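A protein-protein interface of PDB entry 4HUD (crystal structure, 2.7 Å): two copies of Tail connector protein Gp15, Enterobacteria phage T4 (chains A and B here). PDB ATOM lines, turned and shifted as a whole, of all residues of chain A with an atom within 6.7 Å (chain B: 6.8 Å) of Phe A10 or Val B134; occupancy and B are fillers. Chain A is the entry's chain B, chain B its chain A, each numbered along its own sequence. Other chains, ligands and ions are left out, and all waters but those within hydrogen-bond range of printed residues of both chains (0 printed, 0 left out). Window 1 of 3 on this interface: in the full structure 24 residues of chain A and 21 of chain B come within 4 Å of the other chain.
Among the printed residues, pairs that only touch across the chains: Phe A82 with Trp B188, Phe A10 with Phe B131, Ile A114 with Leu B138, Leu A79 with Trp B188, Phe A10 with Val B134, Ser A8 with Phe B131, Met A198 with Leu B138, Met A198 with Glu B135 and Phe A82 with Leu B138.
O of Trp B188 lies within hydrogen-bond range of N of Ile B122 (2.9 Å). OG of Ser A8 is in hydrogen-bond range of N of Phe A10, 3.3 Å away. The backbone NH (N) of Arg A11 is in hydrogen-bond range of the side-chain hydroxyl (OG) of Ser A8 (2.8 Å).
Of chain B, only Phe B131 (3.4 Å), Val B134 (3.8 Å) and Glu B135 (3.1 Å) come within 4 Å of Phe A10. Tyr A13 touches none of the printed residues of chain B. Of the printed residues of chain B, Ile A114 touches Leu B138 (3.7 Å). Printed residues of chain A within 4 Å of Phe B131: Ser A8 and Phe A10. Of chain A, only Phe A10 (3.8 Å) comes within 4 Å of Val B134. The nearest printed residue of chain A that does not touch Leu B138 is Phe A10 (4.1 Å).
Of the 17 printed residues of chain A, 7 touch a printed residue of chain B. Hydrophobic or aromatic side chains of chain B that line the printed part of chain A: Phe B131, Val B134, Leu B138 and Trp B188. Among the printed residues, 12 pairs touch across the chains. Among the printed residues, no Asp or Glu carboxylate lies within 4 Å of a Lys or Arg side-chain nitrogen of the other chain.
The side-chain carboxylate of Glu B135 lies within hydrogen-bond range of the side-chain hydroxyl of Ser A8. The side-chain carboxylate of Glu B135 sits at hydrogen-bond distance from the backbone NH of Ser A9, 2.9 Å away. N of Phe A10 sits at hydrogen-bond distance from OE2 of Glu B135 (3.1 Å).
No position is printed for both chains.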
ATOM      1  N   ASN A   7       6.200 -12.963   3.471  1.00  0.00           N
ATOM      2  CA  ASN A   7       7.032 -13.381   4.600  1.00  0.00           C
ATOM      3  C   ASN A   7       8.456 -12.780   4.597  1.00  0.00           C
ATOM      4  O   ASN A   7       9.310 -13.153   5.411  1.00  0.00           O
ATOM      5  CB  ASN A   7       7.109 -14.908   4.662  1.00  0.00           C
ATOM      6  CG  ASN A   7       5.744 -15.564   4.702  1.00  0.00           C
ATOM      7  OD1 ASN A   7       4.831 -15.109   5.384  1.00  0.00           O
ATOM      8  ND2 ASN A   7       5.600 -16.641   3.957  1.00  0.00           N
ATOM      9  N   SER A   8       8.700 -11.861   3.670  1.00  0.00           N
ATOM     10  CA  SER A   8       9.942 -11.120   3.619  1.00  0.00           C
ATOM     11  C   SER A   8      10.382 -10.635   4.991  1.00  0.00           C
ATOM     12  O   SER A   8       9.609  -9.987   5.699  1.00  0.00           O
ATOM     13  CB  SER A   8       9.789  -9.922   2.691  1.00  0.00           C
ATOM     14  OG  SER A   8      10.741  -8.917   3.021  1.00  0.00           O
ATOM     15  N   SER A   9      11.616 -10.958   5.367  1.00  0.00           N
ATOM     16  CA  SER A   9      12.185 -10.490   6.633  1.00  0.00           C
ATOM     17  C   SER A   9      12.349  -8.957   6.654  1.00  0.00           C
ATOM     18  O   SER A   9      12.104  -8.278   7.667  1.00  0.00           O
ATOM     19  CB  SER A   9      13.531 -11.174   6.897  1.00  0.00           C
ATOM     20  OG  SER A   9      13.357 -12.392   7.595  1.00  0.00           O
ATOM     21  N   PHE A  10      12.782  -8.419   5.524  1.00  0.00           N
ATOM     22  CA  PHE A  10      12.938  -6.983   5.411  1.00  0.00           C
ATOM     23  C   PHE A  10      11.573  -6.352   5.579  1.00  0.00           C
ATOM     24  O   PHE A  10      11.429  -5.396   6.352  1.00  0.00           O
ATOM     25  CB  PHE A  10      13.628  -6.569   4.100  1.00  0.00           C
ATOM     26  CG  PHE A  10      15.126  -6.620   4.159  1.00  0.00           C
ATOM     27  CD1 PHE A  10      15.834  -5.680   4.886  1.00  0.00           C
ATOM     28  CD2 PHE A  10      15.833  -7.602   3.490  1.00  0.00           C
ATOM     29  CE1 PHE A  10      17.220  -5.712   4.941  1.00  0.00           C
ATOM     30  CE2 PHE A  10      17.218  -7.651   3.539  1.00  0.00           C
ATOM     31  CZ  PHE A  10      17.913  -6.700   4.270  1.00  0.00           C
ATOM     32  N   ARG A  11      10.574  -6.893   4.876  1.00  0.00           N
ATOM     33  CA  ARG A  11       9.199  -6.399   5.014  1.00  0.00           C
ATOM     34  C   ARG A  11       8.705  -6.375   6.463  1.00  0.00           C
ATOM     35  O   ARG A  11       8.107  -5.379   6.902  1.00  0.00           O
ATOM     36  CB  ARG A  11       8.218  -7.200   4.150  1.00  0.00           C
ATOM     37  CG  ARG A  11       6.991  -6.396   3.761  1.00  0.00           C
ATOM     38  CD  ARG A  11       5.965  -7.205   3.017  1.00  0.00           C
ATOM     39  NE  ARG A  11       4.647  -6.570   3.073  1.00  0.00           N
ATOM     40  CZ  ARG A  11       4.222  -5.636   2.225  1.00  0.00           C
ATOM     41  NH1 ARG A  11       5.003  -5.230   1.231  1.00  0.00           N
ATOM     42  NH2 ARG A  11       3.005  -5.119   2.357  1.00  0.00           N
ATOM     43  N   ARG A  12       8.969  -7.455   7.202  1.00  0.00           N
ATOM     44  CA  ARG A  12       8.522  -7.524   8.588  1.00  0.00           C
ATOM     45  C   ARG A  12       9.174  -6.451   9.454  1.00  0.00           C
ATOM     46  O   ARG A  12       8.485  -5.757  10.215  1.00  0.00           O
ATOM     47  CB  ARG A  12       8.679  -8.931   9.199  1.00  0.00           C
ATOM     48  CG  ARG A  12       7.562  -9.911   8.734  1.00  0.00           C
ATOM     49  CD  ARG A  12       7.439 -11.235   9.527  1.00  0.00           C
ATOM     50  NE  ARG A  12       8.696 -11.697  10.101  1.00  0.00           N
ATOM     51  CZ  ARG A  12       9.644 -12.336   9.427  1.00  0.00           C
ATOM     52  NH1 ARG A  12       9.483 -12.598   8.137  1.00  0.00           N
ATOM     53  NH2 ARG A  12      10.760 -12.702  10.047  1.00  0.00           N
ATOM     54  N   TYR A  13      10.481  -6.272   9.324  1.00  0.00           N
ATOM     55  CA  TYR A  13      11.091  -5.226  10.129  1.00  0.00           C
ATOM     56  C   TYR A  13      10.583  -3.810   9.750  1.00  0.00           C
ATOM     57  O   TYR A  13      10.290  -2.984  10.630  1.00  0.00           O
ATOM     58  CB  TYR A  13      12.618  -5.362  10.160  1.00  0.00           C
ATOM     59  CG  TYR A  13      13.077  -6.540  10.989  1.00  0.00           C
ATOM     60  CD1 TYR A  13      13.112  -6.465  12.362  1.00  0.00           C
ATOM     61  CD2 TYR A  13      13.447  -7.743  10.393  1.00  0.00           C
ATOM     62  CE1 TYR A  13      13.512  -7.536  13.129  1.00  0.00           C
ATOM     63  CE2 TYR A  13      13.855  -8.829  11.159  1.00  0.00           C
ATOM     64  CZ  TYR A  13      13.877  -8.711  12.530  1.00  0.00           C
ATOM     65  OH  TYR A  13      14.275  -9.764  13.309  1.00  0.00           O
ATOM     66  N   ALA A  14      10.411  -3.563   8.452  1.00  0.00           N
ATOM     67  CA  ALA A  14       9.835  -2.304   7.983  1.00  0.00           C
ATOM     68  C   ALA A  14       8.474  -2.033   8.590  1.00  0.00           C
ATOM     69  O   ALA A  14       8.155  -0.906   8.936  1.00  0.00           O
ATOM     70  CB  ALA A  14       9.736  -2.296   6.482  1.00  0.00           C
ATOM     71  N   THR A  15       7.660  -3.067   8.711  1.00  0.00           N
ATOM     72  CA  THR A  15       6.306  -2.901   9.219  1.00  0.00           C
ATOM     73  C   THR A  15       6.263  -2.752  10.735  1.00  0.00           C
ATOM     74  O   THR A  15       5.497  -1.956  11.269  1.00  0.00           O
ATOM     75  CB  THR A  15       5.454  -4.070   8.787  1.00  0.00           C
ATOM     76  OG1 THR A  15       5.696  -4.292   7.395  1.00  0.00           O
ATOM     77  CG2 THR A  15       3.984  -3.775   8.993  1.00  0.00           C
ATOM     78  N   TYR A  43       6.621   4.645   3.752  1.00  0.00           N
ATOM     79  CA  TYR A  43       7.896   3.955   3.611  1.00  0.00           C
ATOM     80  C   TYR A  43       8.456   4.199   2.222  1.00  0.00           C
ATOM     81  O   TYR A  43       7.884   3.782   1.241  1.00  0.00           O
ATOM     82  CB  TYR A  43       7.710   2.479   3.897  1.00  0.00           C
ATOM     83  CG  TYR A  43       8.979   1.693   4.028  1.00  0.00           C
ATOM     84  CD1 TYR A  43       9.670   1.646   5.224  1.00  0.00           C
ATOM     85  CD2 TYR A  43       9.465   0.951   2.962  1.00  0.00           C
ATOM     86  CE1 TYR A  43      10.820   0.899   5.353  1.00  0.00           C
ATOM     87  CE2 TYR A  43      10.615   0.211   3.076  1.00  0.00           C
ATOM     88  CZ  TYR A  43      11.295   0.185   4.272  1.00  0.00           C
ATOM     89  OH  TYR A  43      12.447  -0.564   4.367  1.00  0.00           O
ATOM     90  N   LEU A  79      14.676   2.245   5.299  1.00  0.00           N
ATOM     91  CA  LEU A  79      15.940   1.561   5.587  1.00  0.00           C
ATOM     92  C   LEU A  79      17.105   2.214   4.810  1.00  0.00           C
ATOM     93  O   LEU A  79      16.972   2.541   3.629  1.00  0.00           O
ATOM     94  CB  LEU A  79      15.807   0.077   5.264  1.00  0.00           C
ATOM     95  CG  LEU A  79      16.941  -0.928   5.451  1.00  0.00           C
ATOM     96  CD1 LEU A  79      17.055  -1.408   6.883  1.00  0.00           C
ATOM     97  CD2 LEU A  79      16.726  -2.090   4.533  1.00  0.00           C
ATOM     98  N   ASP A  81      20.739   1.426   5.950  1.00  0.00           N
ATOM     99  CA  ASP A  81      21.915   0.560   6.068  1.00  0.00           C
ATOM    100  C   ASP A  81      21.619  -0.748   6.812  1.00  0.00           C
ATOM    101  O   ASP A  81      20.663  -0.828   7.564  1.00  0.00           O
ATOM    102  CB  ASP A  81      23.067   1.291   6.754  1.00  0.00           C
ATOM    103  CG  ASP A  81      24.409   0.605   6.533  1.00  0.00           C
ATOM    104  OD1 ASP A  81      25.206   0.533   7.495  1.00  0.00           O
ATOM    105  OD2 ASP A  81      24.667   0.136   5.399  1.00  0.00           O
ATOM    106  N   PHE A  82      22.441  -1.771   6.581  1.00  0.00           N
ATOM    107  CA  PHE A  82      22.403  -2.999   7.389  1.00  0.00           C
ATOM    108  C   PHE A  82      23.777  -3.672   7.358  1.00  0.00           C
ATOM    109  O   PHE A  82      24.533  -3.452   6.434  1.00  0.00           O
ATOM    110  CB  PHE A  82      21.341  -3.973   6.882  1.00  0.00           C
ATOM    111  CG  PHE A  82      21.558  -4.410   5.465  1.00  0.00           C
ATOM    112  CD1 PHE A  82      22.372  -5.491   5.175  1.00  0.00           C
ATOM    113  CD2 PHE A  82      20.963  -3.727   4.420  1.00  0.00           C
ATOM    114  CE1 PHE A  82      22.581  -5.872   3.885  1.00  0.00           C
ATOM    115  CE2 PHE A  82      21.169  -4.110   3.126  1.00  0.00           C
ATOM    116  CZ  PHE A  82      21.980  -5.180   2.859  1.00  0.00           C
ATOM    117  N   ILE A 114      21.348  -9.891  12.525  1.00  0.00           N
ATOM    118  CA  ILE A 114      21.552  -8.817  11.571  1.00  0.00           C
ATOM    119  C   ILE A 114      21.326  -7.501  12.304  1.00  0.00           C
ATOM    120  O   ILE A 114      20.742  -7.459  13.404  1.00  0.00           O
ATOM    121  CB  ILE A 114      20.535  -8.925  10.411  1.00  0.00           C
ATOM    122  CG1 ILE A 114      20.903  -8.042   9.222  1.00  0.00           C
ATOM    123  CG2 ILE A 114      19.160  -8.564  10.890  1.00  0.00           C
ATOM    124  CD1 ILE A 114      19.701  -7.732   8.321  1.00  0.00           C
ATOM    125  N   MET A 116      19.967  -3.523  11.369  1.00  0.00           N
ATOM    126  CA  MET A 116      19.313  -2.727  10.329  1.00  0.00           C
ATOM    127  C   MET A 116      19.157  -1.263  10.758  1.00  0.00           C
ATOM    128  O   MET A 116      18.763  -0.988  11.881  1.00  0.00           O
ATOM    129  CB  MET A 116      17.948  -3.325   9.966  1.00  0.00           C
ATOM    130  CG  MET A 116      18.011  -4.673   9.269  1.00  0.00           C
ATOM    131  SD  MET A 116      16.434  -5.601   9.284  1.00  0.00           S
ATOM    132  CE  MET A 116      16.428  -6.158  10.976  1.00  0.00           C
ATOM    133  N   TYR A 118      17.502   2.510  10.327  1.00  0.00           N
ATOM    134  CA  TYR A 118      16.313   3.161   9.804  1.00  0.00           C
ATOM    135  C   TYR A 118      16.328   4.666  10.013  1.00  0.00           C
ATOM    136  O   TYR A 118      16.618   5.146  11.102  1.00  0.00           O
ATOM    137  CB  TYR A 118      15.057   2.563  10.453  1.00  0.00           C
ATOM    138  CG  TYR A 118      14.677   1.197   9.918  1.00  0.00           C
ATOM    139  CD1 TYR A 118      13.858   1.071   8.812  1.00  0.00           C
ATOM    140  CD2 TYR A 118      15.159   0.034  10.514  1.00  0.00           C
ATOM    141  CE1 TYR A 118      13.520  -0.168   8.320  1.00  0.00           C
ATOM    142  CE2 TYR A 118      14.829  -1.213  10.024  1.00  0.00           C
ATOM    143  CZ  TYR A 118      14.012  -1.306   8.923  1.00  0.00           C
ATOM    144  OH  TYR A 118      13.683  -2.536   8.410  1.00  0.00           O
ATOM    145  N   MET A 198      17.892 -12.330  10.555  1.00  0.00           N
ATOM    146  CA  MET A 198      17.712 -12.633   9.148  1.00  0.00           C
ATOM    147  C   MET A 198      17.777 -14.146   8.910  1.00  0.00           C
ATOM    148  O   MET A 198      18.493 -14.857   9.609  1.00  0.00           O
ATOM    149  CB  MET A 198      18.810 -11.920   8.361  1.00  0.00           C
ATOM    150  CG  MET A 198      18.752 -11.987   6.844  1.00  0.00           C
ATOM    151  SD  MET A 198      17.238 -11.350   6.120  1.00  0.00           S
ATOM    152  CE  MET A 198      16.918  -9.833   7.050  1.00  0.00           C
ATOM    153  N   ILE B  24      19.844 -17.433  -8.487  1.00  0.00           N
ATOM    154  CA  ILE B  24      18.976 -16.705  -7.569  1.00  0.00           C
ATOM    155  C   ILE B  24      17.723 -16.311  -8.316  1.00  0.00           C
ATOM    156  O   ILE B  24      17.792 -15.720  -9.391  1.00  0.00           O
ATOM    157  CB  ILE B  24      19.639 -15.399  -7.072  1.00  0.00           C
ATOM    158  CG1 ILE B  24      20.784 -15.708  -6.112  1.00  0.00           C
ATOM    159  CG2 ILE B  24      18.623 -14.494  -6.420  1.00  0.00           C
ATOM    160  CD1 ILE B  24      21.291 -14.495  -5.389  1.00  0.00           C
ATOM    161  N   ILE B 122      23.302  -5.145  -6.973  1.00  0.00           N
ATOM    162  CA  ILE B 122      21.935  -5.527  -7.293  1.00  0.00           C
ATOM    163  C   ILE B 122      21.072  -4.320  -7.684  1.00  0.00           C
ATOM    164  O   ILE B 122      20.954  -3.355  -6.929  1.00  0.00           O
ATOM    165  CB  ILE B 122      21.310  -6.233  -6.094  1.00  0.00           C
ATOM    166  CG1 ILE B 122      22.338  -7.188  -5.464  1.00  0.00           C
ATOM    167  CG2 ILE B 122      20.029  -6.895  -6.492  1.00  0.00           C
ATOM    168  CD1 ILE B 122      21.840  -7.890  -4.214  1.00  0.00           C
ATOM    169  N   ASP B 129      11.350  -7.088  -5.227  1.00  0.00           N
ATOM    170  CA  ASP B 129      12.437  -7.785  -5.918  1.00  0.00           C
ATOM    171  C   ASP B 129      13.754  -7.763  -5.107  1.00  0.00           C
ATOM    172  O   ASP B 129      14.365  -8.832  -4.859  1.00  0.00           O
ATOM    173  CB  ASP B 129      12.673  -7.169  -7.310  1.00  0.00           C
ATOM    174  CG  ASP B 129      11.684  -7.673  -8.381  1.00  0.00           C
ATOM    175  OD1 ASP B 129      10.725  -8.422  -8.066  1.00  0.00           O
ATOM    176  OD2 ASP B 129      11.884  -7.306  -9.564  1.00  0.00           O
ATOM    177  N   MET B 130      14.151  -6.563  -4.650  1.00  0.00           N
ATOM    178  CA  MET B 130      15.365  -6.415  -3.876  1.00  0.00           C
ATOM    179  C   MET B 130      15.330  -7.251  -2.606  1.00  0.00           C
ATOM    180  O   MET B 130      16.279  -7.973  -2.301  1.00  0.00           O
ATOM    181  CB  MET B 130      15.610  -4.961  -3.482  1.00  0.00           C
ATOM    182  CG  MET B 130      16.369  -4.080  -4.462  1.00  0.00           C
ATOM    183  SD  MET B 130      18.106  -4.483  -4.723  1.00  0.00           S
ATOM    184  CE  MET B 130      18.454  -5.195  -3.143  1.00  0.00           C
ATOM    185  N   PHE B 131      14.235  -7.144  -1.867  1.00  0.00           N
ATOM    186  CA  PHE B 131      14.071  -7.861  -0.603  1.00  0.00           C
ATOM    187  C   PHE B 131      14.258  -9.362  -0.800  1.00  0.00           C
ATOM    188  O   PHE B 131      14.928 -10.031   0.000  1.00  0.00           O
ATOM    189  CB  PHE B 131      12.667  -7.626  -0.056  1.00  0.00           C
ATOM    190  CG  PHE B 131      12.471  -6.277   0.547  1.00  0.00           C
ATOM    191  CD1 PHE B 131      13.545  -5.482   0.848  1.00  0.00           C
ATOM    192  CD2 PHE B 131      11.201  -5.808   0.815  1.00  0.00           C
ATOM    193  CE1 PHE B 131      13.355  -4.264   1.398  1.00  0.00           C
ATOM    194  CE2 PHE B 131      11.010  -4.577   1.366  1.00  0.00           C
ATOM    195  CZ  PHE B 131      12.070  -3.809   1.669  1.00  0.00           C
ATOM    196  N   GLN B 132      13.651  -9.881  -1.864  1.00  0.00           N
ATOM    197  CA  GLN B 132      13.773 -11.295  -2.177  1.00  0.00           C
ATOM    198  C   GLN B 132      15.216 -11.701  -2.407  1.00  0.00           C
ATOM    199  O   GLN B 132      15.762 -12.568  -1.685  1.00  0.00           O
ATOM    200  CB  GLN B 132      12.916 -11.637  -3.397  1.00  0.00           C
ATOM    201  CG  GLN B 132      11.442 -11.810  -3.071  1.00  0.00           C
ATOM    202  CD  GLN B 132      10.620 -12.158  -4.293  1.00  0.00           C
ATOM    203  OE1 GLN B 132      10.699 -13.279  -4.828  1.00  0.00           O
ATOM    204  NE2 GLN B 132       9.785 -11.209  -4.728  1.00  0.00           N
ATOM    205  N   ILE B 133      15.841 -11.033  -3.376  1.00  0.00           N
ATOM    206  CA  ILE B 133      17.230 -11.323  -3.732  1.00  0.00           C
ATOM    207  C   ILE B 133      18.147 -11.301  -2.510  1.00  0.00           C
ATOM    208  O   ILE B 133      18.812 -12.304  -2.178  1.00  0.00           O
ATOM    209  CB  ILE B 133      17.748 -10.340  -4.788  1.00  0.00           C
ATOM    210  CG1 ILE B 133      16.943 -10.464  -6.083  1.00  0.00           C
ATOM    211  CG2 ILE B 133      19.193 -10.600  -5.055  1.00  0.00           C
ATOM    212  CD1 ILE B 133      17.229  -9.380  -7.107  1.00  0.00           C
ATOM    213  N   VAL B 134      18.156 -10.160  -1.822  1.00  0.00           N
ATOM    214  CA  VAL B 134      19.092  -9.951  -0.720  1.00  0.00           C
ATOM    215  C   VAL B 134      18.822 -10.918   0.397  1.00  0.00           C
ATOM    216  O   VAL B 134      19.759 -11.369   1.048  1.00  0.00           O
ATOM    217  CB  VAL B 134      19.081  -8.511  -0.189  1.00  0.00           C
ATOM    218  CG1 VAL B 134      19.991  -8.344   1.054  1.00  0.00           C
ATOM    219  CG2 VAL B 134      19.526  -7.609  -1.266  1.00  0.00           C
ATOM    220  N   GLU B 135      17.553 -11.261   0.605  1.00  0.00           N
ATOM    221  CA  GLU B 135      17.243 -12.281   1.593  1.00  0.00           C
ATOM    222  C   GLU B 135      17.860 -13.617   1.193  1.00  0.00           C
ATOM    223  O   GLU B 135      18.132 -14.448   2.057  1.00  0.00           O
ATOM    224  CB  GLU B 135      15.728 -12.419   1.821  1.00  0.00           C
ATOM    225  CG  GLU B 135      15.182 -11.370   2.805  1.00  0.00           C
ATOM    226  CD  GLU B 135      13.645 -11.339   2.923  1.00  0.00           C
ATOM    227  OE1 GLU B 135      13.006 -12.426   3.031  1.00  0.00           O
ATOM    228  OE2 GLU B 135      13.090 -10.210   2.952  1.00  0.00           O
ATOM    229  N   GLN B 136      18.076 -13.823  -0.110  1.00  0.00           N
ATOM    230  CA  GLN B 136      18.779 -15.041  -0.562  1.00  0.00           C
ATOM    231  C   GLN B 136      20.294 -14.962  -0.502  1.00  0.00           C
ATOM    232  O   GLN B 136      20.965 -15.998  -0.546  1.00  0.00           O
ATOM    233  CB  GLN B 136      18.360 -15.447  -1.969  1.00  0.00           C
ATOM    234  CG  GLN B 136      16.990 -16.089  -2.055  1.00  0.00           C
ATOM    235  CD  GLN B 136      16.527 -16.196  -3.474  1.00  0.00           C
ATOM    236  OE1 GLN B 136      16.955 -17.082  -4.212  1.00  0.00           O
ATOM    237  NE2 GLN B 136      15.659 -15.279  -3.878  1.00  0.00           N
ATOM    238  N   ILE B 137      20.845 -13.752  -0.425  1.00  0.00           N
ATOM    239  CA  ILE B 137      22.303 -13.609  -0.259  1.00  0.00           C
ATOM    240  C   ILE B 137      22.728 -13.499   1.216  1.00  0.00           C
ATOM    241  O   ILE B 137      23.449 -14.347   1.743  1.00  0.00           O
ATOM    242  CB  ILE B 137      22.853 -12.369  -1.020  1.00  0.00           C
ATOM    243  CG1 ILE B 137      22.740 -12.565  -2.531  1.00  0.00           C
ATOM    244  CG2 ILE B 137      24.288 -12.100  -0.646  1.00  0.00           C
ATOM    245  CD1 ILE B 137      22.979 -11.302  -3.306  1.00  0.00           C
ATOM    246  N   LEU B 138      22.262 -12.440   1.859  1.00  0.00           N
ATOM    247  CA  LEU B 138      22.645 -12.043   3.213  1.00  0.00           C
ATOM    248  C   LEU B 138      22.798 -13.078   4.363  1.00  0.00           C
ATOM    249  O   LEU B 138      23.707 -12.933   5.194  1.00  0.00           O
ATOM    250  CB  LEU B 138      21.650 -10.983   3.668  1.00  0.00           C
ATOM    251  CG  LEU B 138      22.113  -9.722   4.356  1.00  0.00           C
ATOM    252  CD1 LEU B 138      20.941  -9.250   5.188  1.00  0.00           C
ATOM    253  CD2 LEU B 138      23.331  -9.975   5.212  1.00  0.00           C
ATOM    254  N   PRO B 139      21.899 -14.081   4.459  1.00  0.00           N
ATOM    255  CA  PRO B 139      22.016 -14.924   5.656  1.00  0.00           C
ATOM    256  C   PRO B 139      23.203 -15.873   5.646  1.00  0.00           C
ATOM    257  O   PRO B 139      23.579 -16.360   6.708  1.00  0.00           O
ATOM    258  CB  PRO B 139      20.695 -15.711   5.675  1.00  0.00           C
ATOM    259  CG  PRO B 139      20.185 -15.645   4.284  1.00  0.00           C
ATOM    260  CD  PRO B 139      20.622 -14.313   3.762  1.00  0.00           C
ATOM    261  N   ILE B 172      23.107   1.355   0.149  1.00  0.00           N
ATOM    262  CA  ILE B 172      21.772   1.526  -0.437  1.00  0.00           C
ATOM    263  C   ILE B 172      21.590   2.870  -1.167  1.00  0.00           C
ATOM    264  O   ILE B 172      21.926   3.920  -0.624  1.00  0.00           O
ATOM    265  CB  ILE B 172      20.711   1.360   0.661  1.00  0.00           C
ATOM    266  CG1 ILE B 172      20.764  -0.067   1.214  1.00  0.00           C
ATOM    267  CG2 ILE B 172      19.319   1.694   0.142  1.00  0.00           C
ATOM    268  CD1 ILE B 172      19.823  -0.321   2.381  1.00  0.00           C
ATOM    269  N   TRP B 188      21.374  -1.544  -4.630  1.00  0.00           N
ATOM    270  CA  TRP B 188      22.058  -1.935  -3.402  1.00  0.00           C
ATOM    271  C   TRP B 188      23.361  -2.637  -3.767  1.00  0.00           C
ATOM    272  O   TRP B 188      23.367  -3.503  -4.638  1.00  0.00           O
ATOM    273  CB  TRP B 188      21.207  -2.936  -2.598  1.00  0.00           C
ATOM    274  CG  TRP B 188      19.940  -2.410  -1.954  1.00  0.00           C
ATOM    275  CD1 TRP B 188      19.243  -1.279  -2.283  1.00  0.00           C
ATOM    276  CD2 TRP B 188      19.259  -2.985  -0.836  1.00  0.00           C
ATOM    277  NE1 TRP B 188      18.152  -1.136  -1.458  1.00  0.00           N
ATOM    278  CE2 TRP B 188      18.135  -2.177  -0.566  1.00  0.00           C
ATOM    279  CE3 TRP B 188      19.474  -4.128  -0.059  1.00  0.00           C
ATOM    280  CZ2 TRP B 188      17.234  -2.468   0.455  1.00  0.00           C
ATOM    281  CZ3 TRP B 188      18.567  -4.424   0.948  1.00  0.00           C
ATOM    282  CH2 TRP B 188      17.464  -3.595   1.197  1.00  0.00           C
ATOM    283  N   LEU B 190      26.670  -4.926  -2.326  1.00  0.00           N
ATOM    284  CA  LEU B 190      27.424  -5.634  -1.293  1.00  0.00           C
ATOM    285  C   LEU B 190      28.938  -5.620  -1.625  1.00  0.00           C
ATOM    286  O   LEU B 190      29.339  -5.714  -2.785  1.00  0.00           O
ATOM    287  CB  LEU B 190      26.926  -7.080  -1.160  1.00  0.00           C
ATOM    288  CG  LEU B 190      25.518  -7.436  -0.629  1.00  0.00           C
ATOM    289  CD1 LEU B 190      25.285  -6.814   0.742  1.00  0.00           C
ATOM    290  CD2 LEU B 190      24.387  -7.041  -1.580  1.00  0.00           C
